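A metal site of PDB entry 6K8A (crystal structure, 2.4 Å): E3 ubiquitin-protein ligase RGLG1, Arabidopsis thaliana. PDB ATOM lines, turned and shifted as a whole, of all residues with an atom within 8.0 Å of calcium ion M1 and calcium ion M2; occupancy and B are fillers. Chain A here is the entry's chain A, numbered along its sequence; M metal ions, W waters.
The backbone carbonyl oxygen (O) of Asp 229 lies within hydrogen-bond range of the side-chain amide nitrogen (NE2) of Gln 264. N of Phe 231 sits close to NE2 of Gln 264 (3.3 Å). O of Ile 203 lies within hydrogen-bond range of N of Gln 232. The side-chain carboxylate of Asp 229 lies close to the guanidinium group of Arg 226, at 3.3 Å. O of Asp 220 sits close to NH2 of Arg 226. The side-chain carboxylate of Glu 260 lies close to the side-chain amide nitrogen of Gln 264 (3.3 Å). OD2 of Asp 229 lies close to N of Ile 15. The side-chain amide nitrogen (NE2) of Gln 232 is in hydrogen-bond range of the backbone carbonyl oxygen (O) of Ser 256 (2.8 Å).
Residues that only touch calcium ion M2: Asp 221. Within 4 Å of calcium ion M2: Asp 220, Asp 221, Gln 232 and Glu 260. The nearest printed residue that does not touch calcium ion M2 is Asp 17 (4.1 Å).
The backbone carbonyl oxygen (O) of Phe 231 is bound to calcium ion M1 (2.3 Å). The side-chain carboxylate (OD1) of Asp 229 is bound to calcium ion M1 (2.4 Å). Calcium ion M1 is bound by O of Asp 220, at 2.4 Å. The side-chain carboxylate (OD1) of Asp 220 is bound to calcium ion M1 (2.4 Å). Calcium ion M1 is bound by OE2 of Glu 260 (2.4 Å). Water W1 is bound to calcium ion M1. Calcium ion M1 is bound by the side-chain carboxylate (OD2) of Asp 229 (2.5 Å). OE1 of Glu 260 is bound to calcium ion M1, 2.5 Å away. Calcium ion M1 has eight donor atoms within binding distance.
Water W2 is bound to calcium ion M2, at 2.3 Å. OE1 of Gln 232 binds calcium ion M2 (2.3 Å). The side-chain carboxylate (OE2) of Glu 260 is bound to calcium ion M2 (2.4 Å). Calcium ion M2 is bound by water W3 (2.4 Å). Water W4 binds calcium ion M2, at 2.5 Å. OD1 of Asp 220 binds calcium ion M2, at 2.6 Å. The side-chain carboxylate (OD2) of Asp 220 is bound to calcium ion M2 (2.6 Å). Slightly farther from calcium ion M2 lies water W1 (3.0 Å).
Water W1 bridges OD1 of Asp 221 (2.7 Å) and O of Ile 15 (2.9 Å). Water W3 bridges OD1 of Asp 17 and NE2 of Gln 232.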
ATOM      1  N   SER A  13     -32.530  21.112 -21.652  1.00  0.00           N
ATOM      2  CA  SER A  13     -31.541  21.645 -20.728  1.00  0.00           C
ATOM      3  C   SER A  13     -30.199  21.850 -21.465  1.00  0.00           C
ATOM      4  O   SER A  13     -29.927  21.143 -22.430  1.00  0.00           O
ATOM      5  CB  SER A  13     -31.379  20.707 -19.521  1.00  0.00           C
ATOM      6  OG  SER A  13     -30.448  21.235 -18.565  1.00  0.00           O
ATOM      7  N   LYS A  14     -29.386  22.799 -20.996  1.00  0.00           N
ATOM      8  CA  LYS A  14     -28.120  23.161 -21.659  1.00  0.00           C
ATOM      9  C   LYS A  14     -26.990  22.176 -21.337  1.00  0.00           C
ATOM     10  O   LYS A  14     -26.888  21.698 -20.223  1.00  0.00           O
ATOM     11  CB  LYS A  14     -27.682  24.581 -21.254  1.00  0.00           C
ATOM     12  CG  LYS A  14     -26.509  25.147 -22.094  1.00  0.00           C
ATOM     13  CD  LYS A  14     -25.696  26.243 -21.353  1.00  0.00           C
ATOM     14  CE  LYS A  14     -24.924  25.684 -20.160  1.00  0.00           C
ATOM     15  NZ  LYS A  14     -23.503  26.188 -20.108  1.00  0.00           N
ATOM     16  N   ILE A  15     -26.147  21.898 -22.338  1.00  0.00           N
ATOM     17  CA  ILE A  15     -25.048  20.950 -22.169  1.00  0.00           C
ATOM     18  C   ILE A  15     -23.727  21.672 -22.076  1.00  0.00           C
ATOM     19  O   ILE A  15     -23.290  22.301 -23.048  1.00  0.00           O
ATOM     20  CB  ILE A  15     -24.981  19.935 -23.329  1.00  0.00           C
ATOM     21  CG1 ILE A  15     -26.265  19.086 -23.388  1.00  0.00           C
ATOM     22  CG2 ILE A  15     -23.762  19.031 -23.189  1.00  0.00           C
ATOM     23  CD1 ILE A  15     -26.268  18.123 -24.537  1.00  0.00           C
ATOM     24  N   SER A  16     -23.074  21.567 -20.914  1.00  0.00           N
ATOM     25  CA  SER A  16     -21.790  22.246 -20.688  1.00  0.00           C
ATOM     26  C   SER A  16     -20.624  21.423 -21.215  1.00  0.00           C
ATOM     27  O   SER A  16     -20.813  20.306 -21.695  1.00  0.00           O
ATOM     28  CB  SER A  16     -21.620  22.525 -19.200  1.00  0.00           C
ATOM     29  OG  SER A  16     -22.742  23.205 -18.679  1.00  0.00           O
ATOM     30  N   ASP A  17     -19.423  21.993 -21.133  1.00  0.00           N
ATOM     31  CA  ASP A  17     -18.191  21.276 -21.483  1.00  0.00           C
ATOM     32  C   ASP A  17     -17.811  20.341 -20.345  1.00  0.00           C
ATOM     33  O   ASP A  17     -17.096  20.735 -19.428  1.00  0.00           O
ATOM     34  CB  ASP A  17     -17.037  22.248 -21.760  1.00  0.00           C
ATOM     35  CG  ASP A  17     -17.222  23.054 -23.048  1.00  0.00           C
ATOM     36  OD1 ASP A  17     -18.221  22.860 -23.776  1.00  0.00           O
ATOM     37  OD2 ASP A  17     -16.343  23.886 -23.332  1.00  0.00           O
ATOM     38  N   ILE A 203     -26.151  18.476 -34.028  1.00  0.00           N
ATOM     39  CA  ILE A 203     -25.617  19.498 -34.936  1.00  0.00           C
ATOM     40  C   ILE A 203     -24.285  20.052 -34.405  1.00  0.00           C
ATOM     41  O   ILE A 203     -24.178  20.428 -33.227  1.00  0.00           O
ATOM     42  CB  ILE A 203     -26.620  20.659 -35.128  1.00  0.00           C
ATOM     43  CG1 ILE A 203     -27.973  20.112 -35.636  1.00  0.00           C
ATOM     44  CG2 ILE A 203     -26.059  21.675 -36.082  1.00  0.00           C
ATOM     45  CD1 ILE A 203     -29.116  21.062 -35.475  1.00  0.00           C
ATOM     46  N   MET A 216     -23.751  32.181 -33.239  1.00  0.00           N
ATOM     47  CA  MET A 216     -23.456  30.759 -33.153  1.00  0.00           C
ATOM     48  C   MET A 216     -23.437  30.316 -31.704  1.00  0.00           C
ATOM     49  O   MET A 216     -23.915  29.228 -31.377  1.00  0.00           O
ATOM     50  CB  MET A 216     -22.139  30.432 -33.826  1.00  0.00           C
ATOM     51  CG  MET A 216     -22.111  30.725 -35.332  1.00  0.00           C
ATOM     52  SD  MET A 216     -23.503  30.052 -36.288  1.00  0.00           S
ATOM     53  CE  MET A 216     -24.690  31.390 -36.270  1.00  0.00           C
ATOM     54  N   GLN A 217     -22.917  31.158 -30.812  1.00  0.00           N
ATOM     55  CA  GLN A 217     -22.889  30.806 -29.396  1.00  0.00           C
ATOM     56  C   GLN A 217     -24.300  30.778 -28.840  1.00  0.00           C
ATOM     57  O   GLN A 217     -24.613  29.961 -27.957  1.00  0.00           O
ATOM     58  CB  GLN A 217     -21.995  31.768 -28.610  1.00  0.00           C
ATOM     59  CG  GLN A 217     -20.510  31.555 -28.917  1.00  0.00           C
ATOM     60  CD  GLN A 217     -19.615  32.689 -28.432  1.00  0.00           C
ATOM     61  OE1 GLN A 217     -20.084  33.790 -28.127  1.00  0.00           O
ATOM     62  NE2 GLN A 217     -18.298  32.424 -28.378  1.00  0.00           N
ATOM     63  N   GLU A 218     -25.172  31.632 -29.364  1.00  0.00           N
ATOM     64  CA  GLU A 218     -26.561  31.603 -28.922  1.00  0.00           C
ATOM     65  C   GLU A 218     -27.277  30.339 -29.407  1.00  0.00           C
ATOM     66  O   GLU A 218     -28.165  29.844 -28.721  1.00  0.00           O
ATOM     67  CB  GLU A 218     -27.297  32.849 -29.395  1.00  0.00           C
ATOM     68  CG  GLU A 218     -27.467  33.880 -28.282  1.00  0.00           C
ATOM     69  CD  GLU A 218     -28.904  34.414 -28.174  1.00  0.00           C
ATOM     70  OE1 GLU A 218     -29.843  33.817 -28.780  1.00  0.00           O
ATOM     71  OE2 GLU A 218     -29.079  35.443 -27.472  1.00  0.00           O
ATOM     72  N   PHE A 219     -26.905  29.809 -30.571  1.00  0.00           N
ATOM     73  CA  PHE A 219     -27.501  28.560 -31.033  1.00  0.00           C
ATOM     74  C   PHE A 219     -27.024  27.420 -30.152  1.00  0.00           C
ATOM     75  O   PHE A 219     -27.772  26.488 -29.855  1.00  0.00           O
ATOM     76  CB  PHE A 219     -27.131  28.243 -32.486  1.00  0.00           C
ATOM     77  CG  PHE A 219     -27.760  29.143 -33.483  1.00  0.00           C
ATOM     78  CD1 PHE A 219     -28.759  30.029 -33.106  1.00  0.00           C
ATOM     79  CD2 PHE A 219     -27.329  29.135 -34.794  1.00  0.00           C
ATOM     80  CE1 PHE A 219     -29.324  30.883 -34.035  1.00  0.00           C
ATOM     81  CE2 PHE A 219     -27.894  29.988 -35.723  1.00  0.00           C
ATOM     82  CZ  PHE A 219     -28.902  30.843 -35.344  1.00  0.00           C
ATOM     83  N   ASP A 220     -25.753  27.515 -29.755  1.00  0.00           N
ATOM     84  CA  ASP A 220     -25.095  26.537 -28.911  1.00  0.00           C
ATOM     85  C   ASP A 220     -25.761  26.478 -27.542  1.00  0.00           C
ATOM     86  O   ASP A 220     -26.091  25.410 -27.057  1.00  0.00           O
ATOM     87  CB  ASP A 220     -23.607  26.894 -28.802  1.00  0.00           C
ATOM     88  CG  ASP A 220     -22.775  25.883 -28.034  1.00  0.00           C
ATOM     89  OD1 ASP A 220     -23.280  24.791 -27.724  1.00  0.00           O
ATOM     90  OD2 ASP A 220     -21.599  26.178 -27.755  1.00  0.00           O
ATOM     91  N   ASP A 221     -26.010  27.642 -26.938  1.00  0.00           N
ATOM     92  CA  ASP A 221     -26.326  27.698 -25.515  1.00  0.00           C
ATOM     93  C   ASP A 221     -27.735  28.158 -25.156  1.00  0.00           C
ATOM     94  O   ASP A 221     -28.168  27.955 -24.027  1.00  0.00           O
ATOM     95  CB  ASP A 221     -25.344  28.630 -24.786  1.00  0.00           C
ATOM     96  CG  ASP A 221     -23.878  28.211 -24.928  1.00  0.00           C
ATOM     97  OD1 ASP A 221     -23.588  26.992 -24.803  1.00  0.00           O
ATOM     98  OD2 ASP A 221     -23.028  29.109 -25.165  1.00  0.00           O
ATOM     99  N   ASN A 222     -28.446  28.813 -26.065  1.00  0.00           N
ATOM    100  CA  ASN A 222     -29.675  29.475 -25.629  1.00  0.00           C
ATOM    101  C   ASN A 222     -30.849  29.485 -26.626  1.00  0.00           C
ATOM    102  O   ASN A 222     -31.108  30.503 -27.279  1.00  0.00           O
ATOM    103  CB  ASN A 222     -29.341  30.912 -25.228  1.00  0.00           C
ATOM    104  CG  ASN A 222     -30.511  31.605 -24.565  1.00  0.00           C
ATOM    105  OD1 ASN A 222     -31.232  31.002 -23.758  1.00  0.00           O
ATOM    106  ND2 ASN A 222     -30.717  32.882 -24.915  1.00  0.00           N
ATOM    107  N   ARG A 226     -36.394  24.307 -27.650  1.00  0.00           N
ATOM    108  CA  ARG A 226     -36.028  23.000 -28.176  1.00  0.00           C
ATOM    109  C   ARG A 226     -36.105  21.900 -27.094  1.00  0.00           C
ATOM    110  O   ARG A 226     -36.044  22.188 -25.901  1.00  0.00           O
ATOM    111  CB  ARG A 226     -34.634  23.045 -28.814  1.00  0.00           C
ATOM    112  CG  ARG A 226     -33.553  23.495 -27.890  1.00  0.00           C
ATOM    113  CD  ARG A 226     -32.188  23.363 -28.539  1.00  0.00           C
ATOM    114  NE  ARG A 226     -31.174  24.022 -27.731  1.00  0.00           N
ATOM    115  CZ  ARG A 226     -29.986  24.413 -28.183  1.00  0.00           C
ATOM    116  NH1 ARG A 226     -29.655  24.187 -29.455  1.00  0.00           N
ATOM    117  NH2 ARG A 226     -29.142  25.022 -27.368  1.00  0.00           N
ATOM    118  N   PHE A 228     -34.072  19.412 -26.421  1.00  0.00           N
ATOM    119  CA  PHE A 228     -32.784  19.203 -25.773  1.00  0.00           C
ATOM    120  C   PHE A 228     -31.720  20.000 -26.516  1.00  0.00           C
ATOM    121  O   PHE A 228     -31.901  20.389 -27.670  1.00  0.00           O
ATOM    122  CB  PHE A 228     -32.412  17.731 -25.751  1.00  0.00           C
ATOM    123  CG  PHE A 228     -32.068  17.154 -27.105  1.00  0.00           C
ATOM    124  CD1 PHE A 228     -33.068  16.765 -27.998  1.00  0.00           C
ATOM    125  CD2 PHE A 228     -30.722  16.981 -27.476  1.00  0.00           C
ATOM    126  CE1 PHE A 228     -32.761  16.220 -29.244  1.00  0.00           C
ATOM    127  CE2 PHE A 228     -30.404  16.443 -28.718  1.00  0.00           C
ATOM    128  CZ  PHE A 228     -31.438  16.050 -29.605  1.00  0.00           C
ATOM    129  N   ASP A 229     -30.596  20.235 -25.853  1.00  0.00           N
ATOM    130  CA  ASP A 229     -29.499  20.985 -26.434  1.00  0.00           C
ATOM    131  C   ASP A 229     -28.863  20.153 -27.553  1.00  0.00           C
ATOM    132  O   ASP A 229     -28.031  19.272 -27.289  1.00  0.00           O
ATOM    133  CB  ASP A 229     -28.488  21.360 -25.349  1.00  0.00           C
ATOM    134  CG  ASP A 229     -27.323  22.178 -25.898  1.00  0.00           C
ATOM    135  OD1 ASP A 229     -27.247  22.373 -27.121  1.00  0.00           O
ATOM    136  OD2 ASP A 229     -26.469  22.595 -25.080  1.00  0.00           O
ATOM    137  N   ASN A 230     -29.244  20.454 -28.796  1.00  0.00           N
ATOM    138  CA  ASN A 230     -28.854  19.657 -29.955  1.00  0.00           C
ATOM    139  C   ASN A 230     -27.779  20.297 -30.837  1.00  0.00           C
ATOM    140  O   ASN A 230     -27.539  19.850 -31.959  1.00  0.00           O
ATOM    141  CB  ASN A 230     -30.078  19.373 -30.819  1.00  0.00           C
ATOM    142  CG  ASN A 230     -30.713  20.661 -31.361  1.00  0.00           C
ATOM    143  OD1 ASN A 230     -30.262  21.761 -31.048  1.00  0.00           O
ATOM    144  ND2 ASN A 230     -31.771  20.522 -32.161  1.00  0.00           N
ATOM    145  N   PHE A 231     -27.132  21.338 -30.315  1.00  0.00           N
ATOM    146  CA  PHE A 231     -26.269  22.195 -31.126  1.00  0.00           C
ATOM    147  C   PHE A 231     -24.944  22.523 -30.434  1.00  0.00           C
ATOM    148  O   PHE A 231     -24.935  23.046 -29.323  1.00  0.00           O
ATOM    149  CB  PHE A 231     -27.005  23.501 -31.452  1.00  0.00           C
ATOM    150  CG  PHE A 231     -26.382  24.302 -32.567  1.00  0.00           C
ATOM    151  CD1 PHE A 231     -25.277  25.112 -32.340  1.00  0.00           C
ATOM    152  CD2 PHE A 231     -26.928  24.278 -33.844  1.00  0.00           C
ATOM    153  CE1 PHE A 231     -24.718  25.869 -33.369  1.00  0.00           C
ATOM    154  CE2 PHE A 231     -26.375  25.037 -34.880  1.00  0.00           C
ATOM    155  CZ  PHE A 231     -25.261  25.835 -34.637  1.00  0.00           C
ATOM    156  N   GLN A 232     -23.839  22.217 -31.097  1.00  0.00           N
ATOM    157  CA  GLN A 232     -22.531  22.576 -30.588  1.00  0.00           C
ATOM    158  C   GLN A 232     -21.803  23.497 -31.564  1.00  0.00           C
ATOM    159  O   GLN A 232     -21.836  23.293 -32.781  1.00  0.00           O
ATOM    160  CB  GLN A 232     -21.681  21.336 -30.309  1.00  0.00           C
ATOM    161  CG  GLN A 232     -20.193  21.602 -30.119  1.00  0.00           C
ATOM    162  CD  GLN A 232     -19.853  22.309 -28.814  1.00  0.00           C
ATOM    163  OE1 GLN A 232     -20.617  23.138 -28.302  1.00  0.00           O
ATOM    164  NE2 GLN A 232     -18.692  21.982 -28.265  1.00  0.00           N
ATOM    165  N   PHE A 233     -21.180  24.541 -31.003  1.00  0.00           N
ATOM    166  CA  PHE A 233     -20.325  25.441 -31.764  1.00  0.00           C
ATOM    167  C   PHE A 233     -18.841  25.187 -31.516  1.00  0.00           C
ATOM    168  O   PHE A 233     -18.385  25.238 -30.372  1.00  0.00           O
ATOM    169  CB  PHE A 233     -20.655  26.894 -31.419  1.00  0.00           C
ATOM    170  CG  PHE A 233     -19.688  27.882 -31.983  1.00  0.00           C
ATOM    171  CD1 PHE A 233     -19.398  27.896 -33.346  1.00  0.00           C
ATOM    172  CD2 PHE A 233     -19.060  28.809 -31.158  1.00  0.00           C
ATOM    173  CE1 PHE A 233     -18.500  28.799 -33.886  1.00  0.00           C
ATOM    174  CE2 PHE A 233     -18.150  29.733 -31.690  1.00  0.00           C
ATOM    175  CZ  PHE A 233     -17.870  29.729 -33.047  1.00  0.00           C
ATOM    176  N   VAL A 234     -18.122  24.902 -32.593  1.00  0.00           N
ATOM    177  CA  VAL A 234     -16.675  24.777 -32.585  1.00  0.00           C
ATOM    178  C   VAL A 234     -16.006  25.960 -33.287  1.00  0.00           C
ATOM    179  O   VAL A 234     -16.111  26.086 -34.511  1.00  0.00           O
ATOM    180  CB  VAL A 234     -16.207  23.500 -33.288  1.00  0.00           C
ATOM    181  CG1 VAL A 234     -14.675  23.462 -33.380  1.00  0.00           C
ATOM    182  CG2 VAL A 234     -16.747  22.273 -32.585  1.00  0.00           C
ATOM    183  N   SER A 256     -13.657  19.402 -29.038  1.00  0.00           N
ATOM    184  CA  SER A 256     -14.707  20.411 -29.156  1.00  0.00           C
ATOM    185  C   SER A 256     -15.931  19.886 -29.930  1.00  0.00           C
ATOM    186  O   SER A 256     -17.063  20.097 -29.527  1.00  0.00           O
ATOM    187  CB  SER A 256     -14.181  21.672 -29.850  1.00  0.00           C
ATOM    188  OG  SER A 256     -13.020  22.143 -29.201  1.00  0.00           O
ATOM    189  N   MET A 259     -17.839  17.216 -27.822  1.00  0.00           N
ATOM    190  CA  MET A 259     -18.136  17.611 -26.444  1.00  0.00           C
ATOM    191  C   MET A 259     -19.565  17.294 -26.012  1.00  0.00           C
ATOM    192  O   MET A 259     -19.786  16.811 -24.894  1.00  0.00           O
ATOM    193  CB  MET A 259     -17.880  19.115 -26.255  1.00  0.00           C
ATOM    194  CG  MET A 259     -17.958  19.574 -24.798  1.00  0.00           C
ATOM    195  SD  MET A 259     -16.637  18.847 -23.775  1.00  0.00           S
ATOM    196  CE  MET A 259     -15.222  19.789 -24.369  1.00  0.00           C
ATOM    197  N   GLU A 260     -20.526  17.565 -26.877  1.00  0.00           N
ATOM    198  CA  GLU A 260     -21.923  17.401 -26.503  1.00  0.00           C
ATOM    199  C   GLU A 260     -22.535  16.107 -27.017  1.00  0.00           C
ATOM    200  O   GLU A 260     -23.707  15.825 -26.749  1.00  0.00           O
ATOM    201  CB  GLU A 260     -22.744  18.594 -26.987  1.00  0.00           C
ATOM    202  CG  GLU A 260     -22.224  19.940 -26.494  1.00  0.00           C
ATOM    203  CD  GLU A 260     -23.205  21.084 -26.774  1.00  0.00           C
ATOM    204  OE1 GLU A 260     -24.376  20.799 -27.086  1.00  0.00           O
ATOM    205  OE2 GLU A 260     -22.814  22.256 -26.661  1.00  0.00           O
ATOM    206  N   GLN A 264     -26.113  14.173 -25.929  1.00  0.00           N
ATOM    207  CA  GLN A 264     -27.100  14.280 -27.014  1.00  0.00           C
ATOM    208  C   GLN A 264     -27.570  12.888 -27.421  1.00  0.00           C
ATOM    209  O   GLN A 264     -28.769  12.654 -27.588  1.00  0.00           O
ATOM    210  CB  GLN A 264     -26.527  15.035 -28.207  1.00  0.00           C
ATOM    211  CG  GLN A 264     -26.626  16.533 -28.068  1.00  0.00           C
ATOM    212  CD  GLN A 264     -25.781  17.270 -29.096  1.00  0.00           C
ATOM    213  OE1 GLN A 264     -25.111  16.634 -29.923  1.00  0.00           O
ATOM    214  NE2 GLN A 264     -25.791  18.609 -29.049  1.00  0.00           N
HETATM  215 CA    CA M   1     -25.009  23.240 -27.013  1.00  0.00          CA
HETATM  216 CA    CA M   2     -21.296  24.081 -26.262  1.00  0.00          CA
HETATM  217  O   HOH W   1     -24.032  24.350 -25.032  1.00  0.00           O
HETATM  218  O   HOH W   2     -21.149  25.962 -24.916  1.00  0.00           O
HETATM  219  O   HOH W   3     -18.874  24.103 -26.211  1.00  0.00           O
HETATM  220  O   HOH W   4     -21.014  22.572 -24.341  1.00  0.00           O
